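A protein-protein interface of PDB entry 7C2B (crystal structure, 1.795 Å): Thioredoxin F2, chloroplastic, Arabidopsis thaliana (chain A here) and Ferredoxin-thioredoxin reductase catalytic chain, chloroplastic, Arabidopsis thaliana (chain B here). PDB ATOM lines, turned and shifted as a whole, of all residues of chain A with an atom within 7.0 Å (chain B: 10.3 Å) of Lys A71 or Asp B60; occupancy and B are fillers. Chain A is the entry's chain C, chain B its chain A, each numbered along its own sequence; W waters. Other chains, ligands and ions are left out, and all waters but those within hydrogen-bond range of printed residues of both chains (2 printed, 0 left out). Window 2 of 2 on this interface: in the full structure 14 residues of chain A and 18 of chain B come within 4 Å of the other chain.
The backbone carbonyl oxygen of Arg A80 lies close to the guanidinium group of Arg B57. The backbone NH of His B58 lies within hydrogen-bond range of the backbone carbonyl oxygen of Arg A80, 3.0 Å away. OD1 of Asp B60 lies within salt-bridge range of NZ of Lys A71, 2.9 Å away.
The backbone carbonyl oxygen (O) of Cys B54 lies within hydrogen-bond range of the side-chain hydroxyl (OH) of Tyr B59 (2.7 Å). O of Tyr B59 sits at hydrogen-bond distance from NZ of Lys B62. O of Asp B60 is in hydrogen-bond range of NZ of Lys B62, 3.3 Å away.
Among the printed residues, pairs that only touch across the chains: Lys A71 with Tyr B59 (3.8 Å), Lys A71 with Lys B62 (3.7 Å), Ala A74 with His B58 (3.8 Å) and Ile A79 with His B58 (3.3 Å).
Lys A71 touches three residues of chain B. Of chain A, only Lys A71 (2.9 Å) comes within 4 Å of Asp B60. No residue of chain B comes within 4 Å of Gln A68. No residue of chain B comes within 4 Å of Asn A70. No residue of chain B comes within 4 Å of Pro A72. Of chain B, only His B58 (3.8 Å) comes within 4 Å of Ala A74. Of the printed residues of chain A, His B58 touches Ala A74, Ile A79 and Arg A80. Of the printed residues of chain B, Arg A80 touches Arg B57 and His B58. Of the printed residues of chain A, Tyr B59 touches Lys A71 (3.8 Å). Printed residues of chain A within 4 Å of Arg B57: Arg A80. The nearest residue of chain B that does not touch Lys A71 is His B58 (4.3 Å).
Printed residues of chain B that touch a printed residue of chain A: Arg B57, His B58, Tyr B59, Asp B60 and Lys B62. Printed residues of chain A that touch a printed residue of chain B: Lys A71, Ala A74, Ile A79 and Arg A80. Hydrophobic or aromatic side chains of chain A within 4 Å of the printed part of chain B: Ala A74 and Ile A79. Along chain A the printed residues that touch a printed residue of chain B span positions 71 to 80. Among the printed residues, Asp or Glu carboxylates within 4 Å of a Lys or Arg side-chain nitrogen of the other chain: Lys A71 with Asp B60.
Water W1 bridges ND1 of His B58 and O of Cys A66. Water W2 lies within hydrogen-bond range of OD1 of Asp B60 (2.7 Å) and NZ of Lys A75 (3.5 Å).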
ATOM      1  N   LYS A  15      19.172 -18.383  39.224  1.00  0.00           N
ATOM      2  CA  LYS A  15      20.554 -17.929  39.116  1.00  0.00           C
ATOM      3  C   LYS A  15      21.129 -17.460  40.444  1.00  0.00           C
ATOM      4  O   LYS A  15      22.351 -17.389  40.579  1.00  0.00           O
ATOM      5  CB  LYS A  15      20.663 -16.801  38.098  1.00  0.00           C
ATOM      6  CG  LYS A  15      19.951 -15.524  38.524  1.00  0.00           C
ATOM      7  CD  LYS A  15      20.278 -14.391  37.567  1.00  0.00           C
ATOM      8  CE  LYS A  15      19.932 -13.034  38.153  1.00  0.00           C
ATOM      9  NZ  LYS A  15      18.937 -12.367  37.263  1.00  0.00           N
ATOM     10  N   ASP A  65      15.302 -23.732  35.187  1.00  0.00           N
ATOM     11  CA  ASP A  65      14.652 -23.283  33.954  1.00  0.00           C
ATOM     12  C   ASP A  65      15.588 -22.299  33.261  1.00  0.00           C
ATOM     13  O   ASP A  65      15.834 -21.208  33.778  1.00  0.00           O
ATOM     14  CB  ASP A  65      13.302 -22.650  34.291  1.00  0.00           C
ATOM     15  CG  ASP A  65      12.510 -22.214  33.065  1.00  0.00           C
ATOM     16  OD1 ASP A  65      13.044 -22.233  31.929  1.00  0.00           O
ATOM     17  OD2 ASP A  65      11.324 -21.840  33.249  1.00  0.00           O
ATOM     18  N   CYS A  66      16.130 -22.684  32.105  1.00  0.00           N
ATOM     19  CA  CYS A  66      17.068 -21.833  31.372  1.00  0.00           C
ATOM     20  C   CYS A  66      16.305 -20.826  30.506  1.00  0.00           C
ATOM     21  O   CYS A  66      16.227 -20.924  29.281  1.00  0.00           O
ATOM     22  CB  CYS A  66      18.034 -22.687  30.563  1.00  0.00           C
ATOM     23  SG  CYS A  66      19.056 -23.750  31.643  1.00  0.00           S
ATOM     24  N   ASN A  67      15.738 -19.835  31.183  1.00  0.00           N
ATOM     25  CA  ASN A  67      14.988 -18.767  30.537  1.00  0.00           C
ATOM     26  C   ASN A  67      15.819 -17.485  30.554  1.00  0.00           C
ATOM     27  O   ASN A  67      16.997 -17.485  30.924  1.00  0.00           O
ATOM     28  CB  ASN A  67      13.630 -18.590  31.228  1.00  0.00           C
ATOM     29  CG  ASN A  67      13.763 -18.270  32.722  1.00  0.00           C
ATOM     30  OD1 ASN A  67      14.834 -17.882  33.200  1.00  0.00           O
ATOM     31  ND2 ASN A  67      12.667 -18.415  33.457  1.00  0.00           N
ATOM     32  N   GLN A  68      15.183 -16.371  30.175  1.00  0.00           N
ATOM     33  CA  GLN A  68      15.902 -15.109  30.097  1.00  0.00           C
ATOM     34  C   GLN A  68      16.404 -14.667  31.465  1.00  0.00           C
ATOM     35  O   GLN A  68      17.545 -14.211  31.591  1.00  0.00           O
ATOM     36  CB  GLN A  68      15.003 -14.036  29.468  1.00  0.00           C
ATOM     37  CG  GLN A  68      15.719 -12.731  29.172  1.00  0.00           C
ATOM     38  CD  GLN A  68      17.028 -12.932  28.427  1.00  0.00           C
ATOM     39  OE1 GLN A  68      17.044 -13.417  27.292  1.00  0.00           O
ATOM     40  NE2 GLN A  68      18.141 -12.560  29.068  1.00  0.00           N
ATOM     41  N   ASP A  69      15.575 -14.802  32.506  1.00  0.00           N
ATOM     42  CA  ASP A  69      15.990 -14.375  33.840  1.00  0.00           C
ATOM     43  C   ASP A  69      17.236 -15.128  34.307  1.00  0.00           C
ATOM     44  O   ASP A  69      18.113 -14.548  34.960  1.00  0.00           O
ATOM     45  CB  ASP A  69      14.859 -14.588  34.848  1.00  0.00           C
ATOM     46  CG  ASP A  69      13.706 -13.603  34.666  1.00  0.00           C
ATOM     47  OD1 ASP A  69      13.923 -12.502  34.112  1.00  0.00           O
ATOM     48  OD2 ASP A  69      12.579 -13.939  35.092  1.00  0.00           O
ATOM     49  N   ASN A  70      17.327 -16.420  33.996  1.00  0.00           N
ATOM     50  CA  ASN A  70      18.396 -17.267  34.523  1.00  0.00           C
ATOM     51  C   ASN A  70      19.557 -17.426  33.557  1.00  0.00           C
ATOM     52  O   ASN A  70      20.485 -18.197  33.829  1.00  0.00           O
ATOM     53  CB  ASN A  70      17.833 -18.636  34.897  1.00  0.00           C
ATOM     54  CG  ASN A  70      16.951 -18.569  36.112  1.00  0.00           C
ATOM     55  OD1 ASN A  70      17.198 -17.774  37.008  1.00  0.00           O
ATOM     56  ND2 ASN A  70      15.914 -19.389  36.149  1.00  0.00           N
ATOM     57  N   LYS A  71      19.536 -16.699  32.451  1.00  0.00           N
ATOM     58  CA  LYS A  71      20.576 -16.826  31.439  1.00  0.00           C
ATOM     59  C   LYS A  71      21.996 -16.648  31.973  1.00  0.00           C
ATOM     60  O   LYS A  71      22.878 -17.398  31.527  1.00  0.00           O
ATOM     61  CB  LYS A  71      20.291 -15.831  30.306  1.00  0.00           C
ATOM     62  CG  LYS A  71      21.144 -16.038  29.067  1.00  0.00           C
ATOM     63  CD  LYS A  71      20.843 -14.944  28.035  1.00  0.00           C
ATOM     64  CE  LYS A  71      21.598 -15.166  26.736  1.00  0.00           C
ATOM     65  NZ  LYS A  71      23.066 -15.190  26.939  1.00  0.00           N
ATOM     66  N   PRO A  72      22.291 -15.723  32.903  1.00  0.00           N
ATOM     67  CA  PRO A  72      23.676 -15.642  33.400  1.00  0.00           C
ATOM     68  C   PRO A  72      24.185 -16.957  33.968  1.00  0.00           C
ATOM     69  O   PRO A  72      25.347 -17.316  33.746  1.00  0.00           O
ATOM     70  CB  PRO A  72      23.602 -14.539  34.469  1.00  0.00           C
ATOM     71  CG  PRO A  72      22.465 -13.678  34.038  1.00  0.00           C
ATOM     72  CD  PRO A  72      21.450 -14.646  33.464  1.00  0.00           C
ATOM     73  N   LEU A  73      23.342 -17.695  34.685  1.00  0.00           N
ATOM     74  CA  LEU A  73      23.776 -18.977  35.233  1.00  0.00           C
ATOM     75  C   LEU A  73      23.835 -20.040  34.144  1.00  0.00           C
ATOM     76  O   LEU A  73      24.751 -20.860  34.127  1.00  0.00           O
ATOM     77  CB  LEU A  73      22.843 -19.416  36.369  1.00  0.00           C
ATOM     78  CG  LEU A  73      23.125 -20.783  36.988  1.00  0.00           C
ATOM     79  CD1 LEU A  73      24.551 -20.853  37.540  1.00  0.00           C
ATOM     80  CD2 LEU A  73      22.130 -21.113  38.092  1.00  0.00           C
ATOM     81  N   ALA A  74      22.869 -20.046  33.224  1.00  0.00           N
ATOM     82  CA  ALA A  74      22.967 -20.953  32.084  1.00  0.00           C
ATOM     83  C   ALA A  74      24.282 -20.754  31.332  1.00  0.00           C
ATOM     84  O   ALA A  74      24.958 -21.728  30.968  1.00  0.00           O
ATOM     85  CB  ALA A  74      21.775 -20.751  31.146  1.00  0.00           C
ATOM     86  N   LYS A  75      24.666 -19.498  31.095  1.00  0.00           N
ATOM     87  CA  LYS A  75      25.904 -19.233  30.369  1.00  0.00           C
ATOM     88  C   LYS A  75      27.119 -19.682  31.170  1.00  0.00           C
ATOM     89  O   LYS A  75      28.074 -20.230  30.610  1.00  0.00           O
ATOM     90  CB  LYS A  75      26.012 -17.745  30.044  1.00  0.00           C
ATOM     91  CG  LYS A  75      27.287 -17.369  29.296  1.00  0.00           C
ATOM     92  CD  LYS A  75      27.283 -15.897  28.944  1.00  0.00           C
ATOM     93  CE  LYS A  75      28.290 -15.588  27.843  1.00  0.00           C
ATOM     94  NZ  LYS A  75      29.152 -14.433  28.213  1.00  0.00           N
ATOM     95  N   GLU A  76      27.105 -19.444  32.479  1.00  0.00           N
ATOM     96  CA  GLU A  76      28.239 -19.844  33.310  1.00  0.00           C
ATOM     97  C   GLU A  76      28.390 -21.364  33.362  1.00  0.00           C
ATOM     98  O   GLU A  76      29.504 -21.887  33.242  1.00  0.00           O
ATOM     99  CB  GLU A  76      28.078 -19.266  34.714  1.00  0.00           C
ATOM    100  CG  GLU A  76      29.120 -19.758  35.711  1.00  0.00           C
ATOM    101  CD  GLU A  76      29.156 -18.902  36.949  1.00  0.00           C
ATOM    102  OE1 GLU A  76      28.255 -19.055  37.811  1.00  0.00           O
ATOM    103  OE2 GLU A  76      30.078 -18.069  37.055  1.00  0.00           O
ATOM    104  N   LEU A  77      27.282 -22.096  33.519  1.00  0.00           N
ATOM    105  CA  LEU A  77      27.380 -23.553  33.584  1.00  0.00           C
ATOM    106  C   LEU A  77      27.698 -24.156  32.224  1.00  0.00           C
ATOM    107  O   LEU A  77      28.342 -25.207  32.149  1.00  0.00           O
ATOM    108  CB  LEU A  77      26.078 -24.153  34.114  1.00  0.00           C
ATOM    109  CG  LEU A  77      25.788 -23.960  35.600  1.00  0.00           C
ATOM    110  CD1 LEU A  77      24.342 -24.343  35.891  1.00  0.00           C
ATOM    111  CD2 LEU A  77      26.765 -24.778  36.468  1.00  0.00           C
ATOM    112  N   ILE A  79      25.467 -24.552  28.430  1.00  0.00           N
ATOM    113  CA  ILE A  79      24.406 -25.429  27.928  1.00  0.00           C
ATOM    114  C   ILE A  79      24.151 -25.095  26.463  1.00  0.00           C
ATOM    115  O   ILE A  79      24.091 -23.918  26.087  1.00  0.00           O
ATOM    116  CB  ILE A  79      23.107 -25.327  28.762  1.00  0.00           C
ATOM    117  CG1 ILE A  79      21.983 -26.159  28.102  1.00  0.00           C
ATOM    118  CG2 ILE A  79      22.693 -23.875  28.934  1.00  0.00           C
ATOM    119  CD1 ILE A  79      20.705 -26.283  28.929  1.00  0.00           C
ATOM    120  N   ARG A  80      24.059 -26.141  25.633  1.00  0.00           N
ATOM    121  CA  ARG A  80      23.702 -26.002  24.224  1.00  0.00           C
ATOM    122  C   ARG A  80      22.529 -26.917  23.887  1.00  0.00           C
ATOM    123  O   ARG A  80      21.560 -26.484  23.267  1.00  0.00           O
ATOM    124  CB  ARG A  80      24.915 -26.310  23.336  1.00  0.00           C
ATOM    125  CG  ARG A  80      25.975 -25.182  23.313  1.00  0.00           C
ATOM    126  CD  ARG A  80      25.356 -23.905  22.719  1.00  0.00           C
ATOM    127  NE  ARG A  80      26.267 -22.759  22.614  1.00  0.00           N
ATOM    128  CZ  ARG A  80      26.217 -21.690  23.409  1.00  0.00           C
ATOM    129  NH1 ARG A  80      27.067 -20.684  23.240  1.00  0.00           N
ATOM    130  NH2 ARG A  80      25.321 -21.630  24.388  1.00  0.00           N
ATOM    131  N   TYR B  49      11.197 -13.968  19.006  1.00  0.00           N
ATOM    132  CA  TYR B  49      12.436 -13.719  18.285  1.00  0.00           C
ATOM    133  C   TYR B  49      12.248 -13.518  16.792  1.00  0.00           C
ATOM    134  O   TYR B  49      13.206 -13.130  16.113  1.00  0.00           O
ATOM    135  CB  TYR B  49      13.427 -14.874  18.505  1.00  0.00           C
ATOM    136  CG  TYR B  49      13.654 -15.235  19.948  1.00  0.00           C
ATOM    137  CD1 TYR B  49      13.876 -14.249  20.903  1.00  0.00           C
ATOM    138  CD2 TYR B  49      13.669 -16.565  20.358  1.00  0.00           C
ATOM    139  CE1 TYR B  49      14.097 -14.566  22.228  1.00  0.00           C
ATOM    140  CE2 TYR B  49      13.891 -16.900  21.698  1.00  0.00           C
ATOM    141  CZ  TYR B  49      14.104 -15.891  22.623  1.00  0.00           C
ATOM    142  OH  TYR B  49      14.324 -16.203  23.945  1.00  0.00           O
ATOM    143  N   LEU B  53      13.040 -20.820  16.308  1.00  0.00           N
ATOM    144  CA  LEU B  53      14.245 -21.514  16.732  1.00  0.00           C
ATOM    145  C   LEU B  53      13.870 -22.760  17.520  1.00  0.00           C
ATOM    146  O   LEU B  53      12.890 -22.776  18.270  1.00  0.00           O
ATOM    147  CB  LEU B  53      15.140 -20.610  17.593  1.00  0.00           C
ATOM    148  CG  LEU B  53      15.695 -19.361  16.908  1.00  0.00           C
ATOM    149  CD1 LEU B  53      16.489 -18.536  17.900  1.00  0.00           C
ATOM    150  CD2 LEU B  53      16.562 -19.754  15.725  1.00  0.00           C
ATOM    151  N   CYS B  54      14.670 -23.798  17.343  1.00  0.00           N
ATOM    152  CA  CYS B  54      14.531 -25.057  18.053  1.00  0.00           C
ATOM    153  C   CYS B  54      14.303 -24.807  19.535  1.00  0.00           C
ATOM    154  O   CYS B  54      15.119 -24.135  20.173  1.00  0.00           O
ATOM    155  CB  CYS B  54      15.782 -25.910  17.872  1.00  0.00           C
ATOM    156  SG  CYS B  54      15.528 -27.542  18.567  1.00  0.00           S
ATOM    157  N   ARG B  57      17.191 -26.221  22.206  1.00  0.00           N
ATOM    158  CA  ARG B  57      18.548 -25.689  22.167  1.00  0.00           C
ATOM    159  C   ARG B  57      18.598 -24.438  23.029  1.00  0.00           C
ATOM    160  O   ARG B  57      17.586 -23.747  23.196  1.00  0.00           O
ATOM    161  CB  ARG B  57      18.983 -25.347  20.720  1.00  0.00           C
ATOM    162  CG  ARG B  57      18.994 -26.535  19.761  1.00  0.00           C
ATOM    163  CD  ARG B  57      20.151 -27.484  20.039  1.00  0.00           C
ATOM    164  NE  ARG B  57      21.440 -26.806  19.967  1.00  0.00           N
ATOM    165  CZ  ARG B  57      22.618 -27.423  19.947  1.00  0.00           C
ATOM    166  NH1 ARG B  57      22.679 -28.746  19.993  1.00  0.00           N
ATOM    167  NH2 ARG B  57      23.737 -26.715  19.879  1.00  0.00           N
ATOM    168  N   HIS B  58      19.773 -24.150  23.589  1.00  0.00           N
ATOM    169  CA  HIS B  58      19.994 -22.894  24.297  1.00  0.00           C
ATOM    170  C   HIS B  58      20.872 -21.983  23.450  1.00  0.00           C
ATOM    171  O   HIS B  58      21.840 -22.441  22.842  1.00  0.00           O
ATOM    172  CB  HIS B  58      20.655 -23.115  25.659  1.00  0.00           C
ATOM    173  CG  HIS B  58      21.059 -21.840  26.328  1.00  0.00           C
ATOM    174  ND1 HIS B  58      20.178 -21.081  27.067  1.00  0.00           N
ATOM    175  CD2 HIS B  58      22.231 -21.162  26.319  1.00  0.00           C
ATOM    176  CE1 HIS B  58      20.803 -20.009  27.522  1.00  0.00           C
ATOM    177  NE2 HIS B  58      22.053 -20.036  27.085  1.00  0.00           N
ATOM    178  N   TYR B  59      20.525 -20.695  23.412  1.00  0.00           N
ATOM    179  CA  TYR B  59      21.182 -19.724  22.552  1.00  0.00           C
ATOM    180  C   TYR B  59      21.725 -18.549  23.355  1.00  0.00           C
ATOM    181  O   TYR B  59      21.130 -18.124  24.349  1.00  0.00           O
ATOM    182  CB  TYR B  59      20.221 -19.180  21.498  1.00  0.00           C
ATOM    183  CG  TYR B  59      19.434 -20.251  20.791  1.00  0.00           C
ATOM    184  CD1 TYR B  59      20.035 -21.052  19.825  1.00  0.00           C
ATOM    185  CD2 TYR B  59      18.100 -20.472  21.094  1.00  0.00           C
ATOM    186  CE1 TYR B  59      19.320 -22.050  19.173  1.00  0.00           C
ATOM    187  CE2 TYR B  59      17.373 -21.471  20.440  1.00  0.00           C
ATOM    188  CZ  TYR B  59      17.988 -22.247  19.477  1.00  0.00           C
ATOM    189  OH  TYR B  59      17.268 -23.237  18.815  1.00  0.00           O
ATOM    190  N   ASP B  60      22.846 -18.006  22.884  1.00  0.00           N
ATOM    191  CA  ASP B  60      23.365 -16.753  23.416  1.00  0.00           C
ATOM    192  C   ASP B  60      22.619 -15.583  22.784  1.00  0.00           C
ATOM    193  O   ASP B  60      21.663 -15.060  23.373  1.00  0.00           O
ATOM    194  CB  ASP B  60      24.868 -16.654  23.162  1.00  0.00           C
ATOM    195  CG  ASP B  60      25.507 -15.488  23.890  1.00  0.00           C
ATOM    196  OD1 ASP B  60      24.784 -14.741  24.588  1.00  0.00           O
ATOM    197  OD2 ASP B  60      26.733 -15.321  23.758  1.00  0.00           O
ATOM    198  N   ASP B  61      23.013 -15.184  21.575  1.00  0.00           N
ATOM    199  CA  ASP B  61      22.380 -14.053  20.897  1.00  0.00           C
ATOM    200  C   ASP B  61      21.265 -14.564  19.992  1.00  0.00           C
ATOM    201  O   ASP B  61      21.538 -15.135  18.932  1.00  0.00           O
ATOM    202  CB  ASP B  61      23.402 -13.260  20.091  1.00  0.00           C
ATOM    203  CG  ASP B  61      22.842 -11.944  19.592  1.00  0.00           C
ATOM    204  OD1 ASP B  61      21.946 -11.956  18.735  1.00  0.00           O
ATOM    205  OD2 ASP B  61      23.268 -10.889  20.099  1.00  0.00           O
ATOM    206  N   LYS B  62      20.010 -14.337  20.395  1.00  0.00           N
ATOM    207  CA  LYS B  62      18.876 -14.853  19.630  1.00  0.00           C
ATOM    208  C   LYS B  62      18.818 -14.248  18.230  1.00  0.00           C
ATOM    209  O   LYS B  62      18.536 -14.954  17.256  1.00  0.00           O
ATOM    210  CB  LYS B  62      17.565 -14.581  20.374  1.00  0.00           C
ATOM    211  CG  LYS B  62      17.617 -14.843  21.881  1.00  0.00           C
ATOM    212  CD  LYS B  62      17.893 -16.308  22.188  1.00  0.00           C
ATOM    213  CE  LYS B  62      17.651 -16.629  23.666  1.00  0.00           C
ATOM    214  NZ  LYS B  62      18.777 -16.220  24.577  1.00  0.00           N
ATOM    215  N   ALA B  63      19.078 -12.942  18.107  1.00  0.00           N
ATOM    216  CA  ALA B  63      18.942 -12.311  16.793  1.00  0.00           C
ATOM    217  C   ALA B  63      19.968 -12.856  15.816  1.00  0.00           C
ATOM    218  O   ALA B  63      19.673 -13.001  14.619  1.00  0.00           O
ATOM    219  CB  ALA B  63      19.066 -10.786  16.907  1.00  0.00           C
ATOM    220  N   ALA B  64      21.160 -13.199  16.310  1.00  0.00           N
ATOM    221  CA  ALA B  64      22.179 -13.772  15.442  1.00  0.00           C
ATOM    222  C   ALA B  64      21.807 -15.188  15.020  1.00  0.00           C
ATOM    223  O   ALA B  64      22.037 -15.580  13.867  1.00  0.00           O
ATOM    224  CB  ALA B  64      23.540 -13.748  16.143  1.00  0.00           C
ATOM    225  N   GLU B  65      21.237 -15.971  15.935  1.00  0.00           N
ATOM    226  CA  GLU B  65      20.772 -17.306  15.571  1.00  0.00           C
ATOM    227  C   GLU B  65      19.637 -17.241  14.548  1.00  0.00           C
ATOM    228  O   GLU B  65      19.605 -18.034  13.601  1.00  0.00           O
ATOM    229  CB  GLU B  65      20.335 -18.058  16.827  1.00  0.00           C
ATOM    230  CG  GLU B  65      21.489 -18.349  17.791  1.00  0.00           C
ATOM    231  CD  GLU B  65      22.310 -19.560  17.382  1.00  0.00           C
ATOM    232  OE1 GLU B  65      21.961 -20.223  16.380  1.00  0.00           O
ATOM    233  OE2 GLU B  65      23.308 -19.861  18.073  1.00  0.00           O
ATOM    234  N   VAL B  66      18.709 -16.295  14.710  1.00  0.00           N
ATOM    235  CA  VAL B  66      17.641 -16.126  13.721  1.00  0.00           C
ATOM    236  C   VAL B  66      18.231 -15.791  12.358  1.00  0.00           C
ATOM    237  O   VAL B  66      17.839 -16.363  11.332  1.00  0.00           O
ATOM    238  CB  VAL B  66      16.641 -15.048  14.185  1.00  0.00           C
ATOM    239  CG1 VAL B  66      15.777 -14.543  13.006  1.00  0.00           C
ATOM    240  CG2 VAL B  66      15.756 -15.579  15.290  1.00  0.00           C
ATOM    241  N   TRP B  71      19.537 -23.294  13.375  1.00  0.00           N
ATOM    242  CA  TRP B  71      18.622 -23.908  14.320  1.00  0.00           C
ATOM    243  C   TRP B  71      17.185 -23.440  14.131  1.00  0.00           C
ATOM    244  O   TRP B  71      16.345 -23.730  14.981  1.00  0.00           O
ATOM    245  CB  TRP B  71      19.072 -23.647  15.756  1.00  0.00           C
ATOM    246  CG  TRP B  71      20.257 -24.459  16.141  1.00  0.00           C
ATOM    247  CD1 TRP B  71      21.498 -23.987  16.478  1.00  0.00           C
ATOM    248  CD2 TRP B  71      20.338 -25.892  16.217  1.00  0.00           C
ATOM    249  NE1 TRP B  71      22.333 -25.030  16.764  1.00  0.00           N
ATOM    250  CE2 TRP B  71      21.654 -26.212  16.597  1.00  0.00           C
ATOM    251  CE3 TRP B  71      19.424 -26.930  15.992  1.00  0.00           C
ATOM    252  CZ2 TRP B  71      22.085 -27.531  16.774  1.00  0.00           C
ATOM    253  CZ3 TRP B  71      19.846 -28.247  16.156  1.00  0.00           C
ATOM    254  CH2 TRP B  71      21.166 -28.537  16.549  1.00  0.00           C
HETATM  255  O   HOH W   1      17.691 -21.820  27.193  1.00  0.00           O
HETATM  256  O   HOH W   2      26.247 -13.568  26.482  1.00  0.00           O
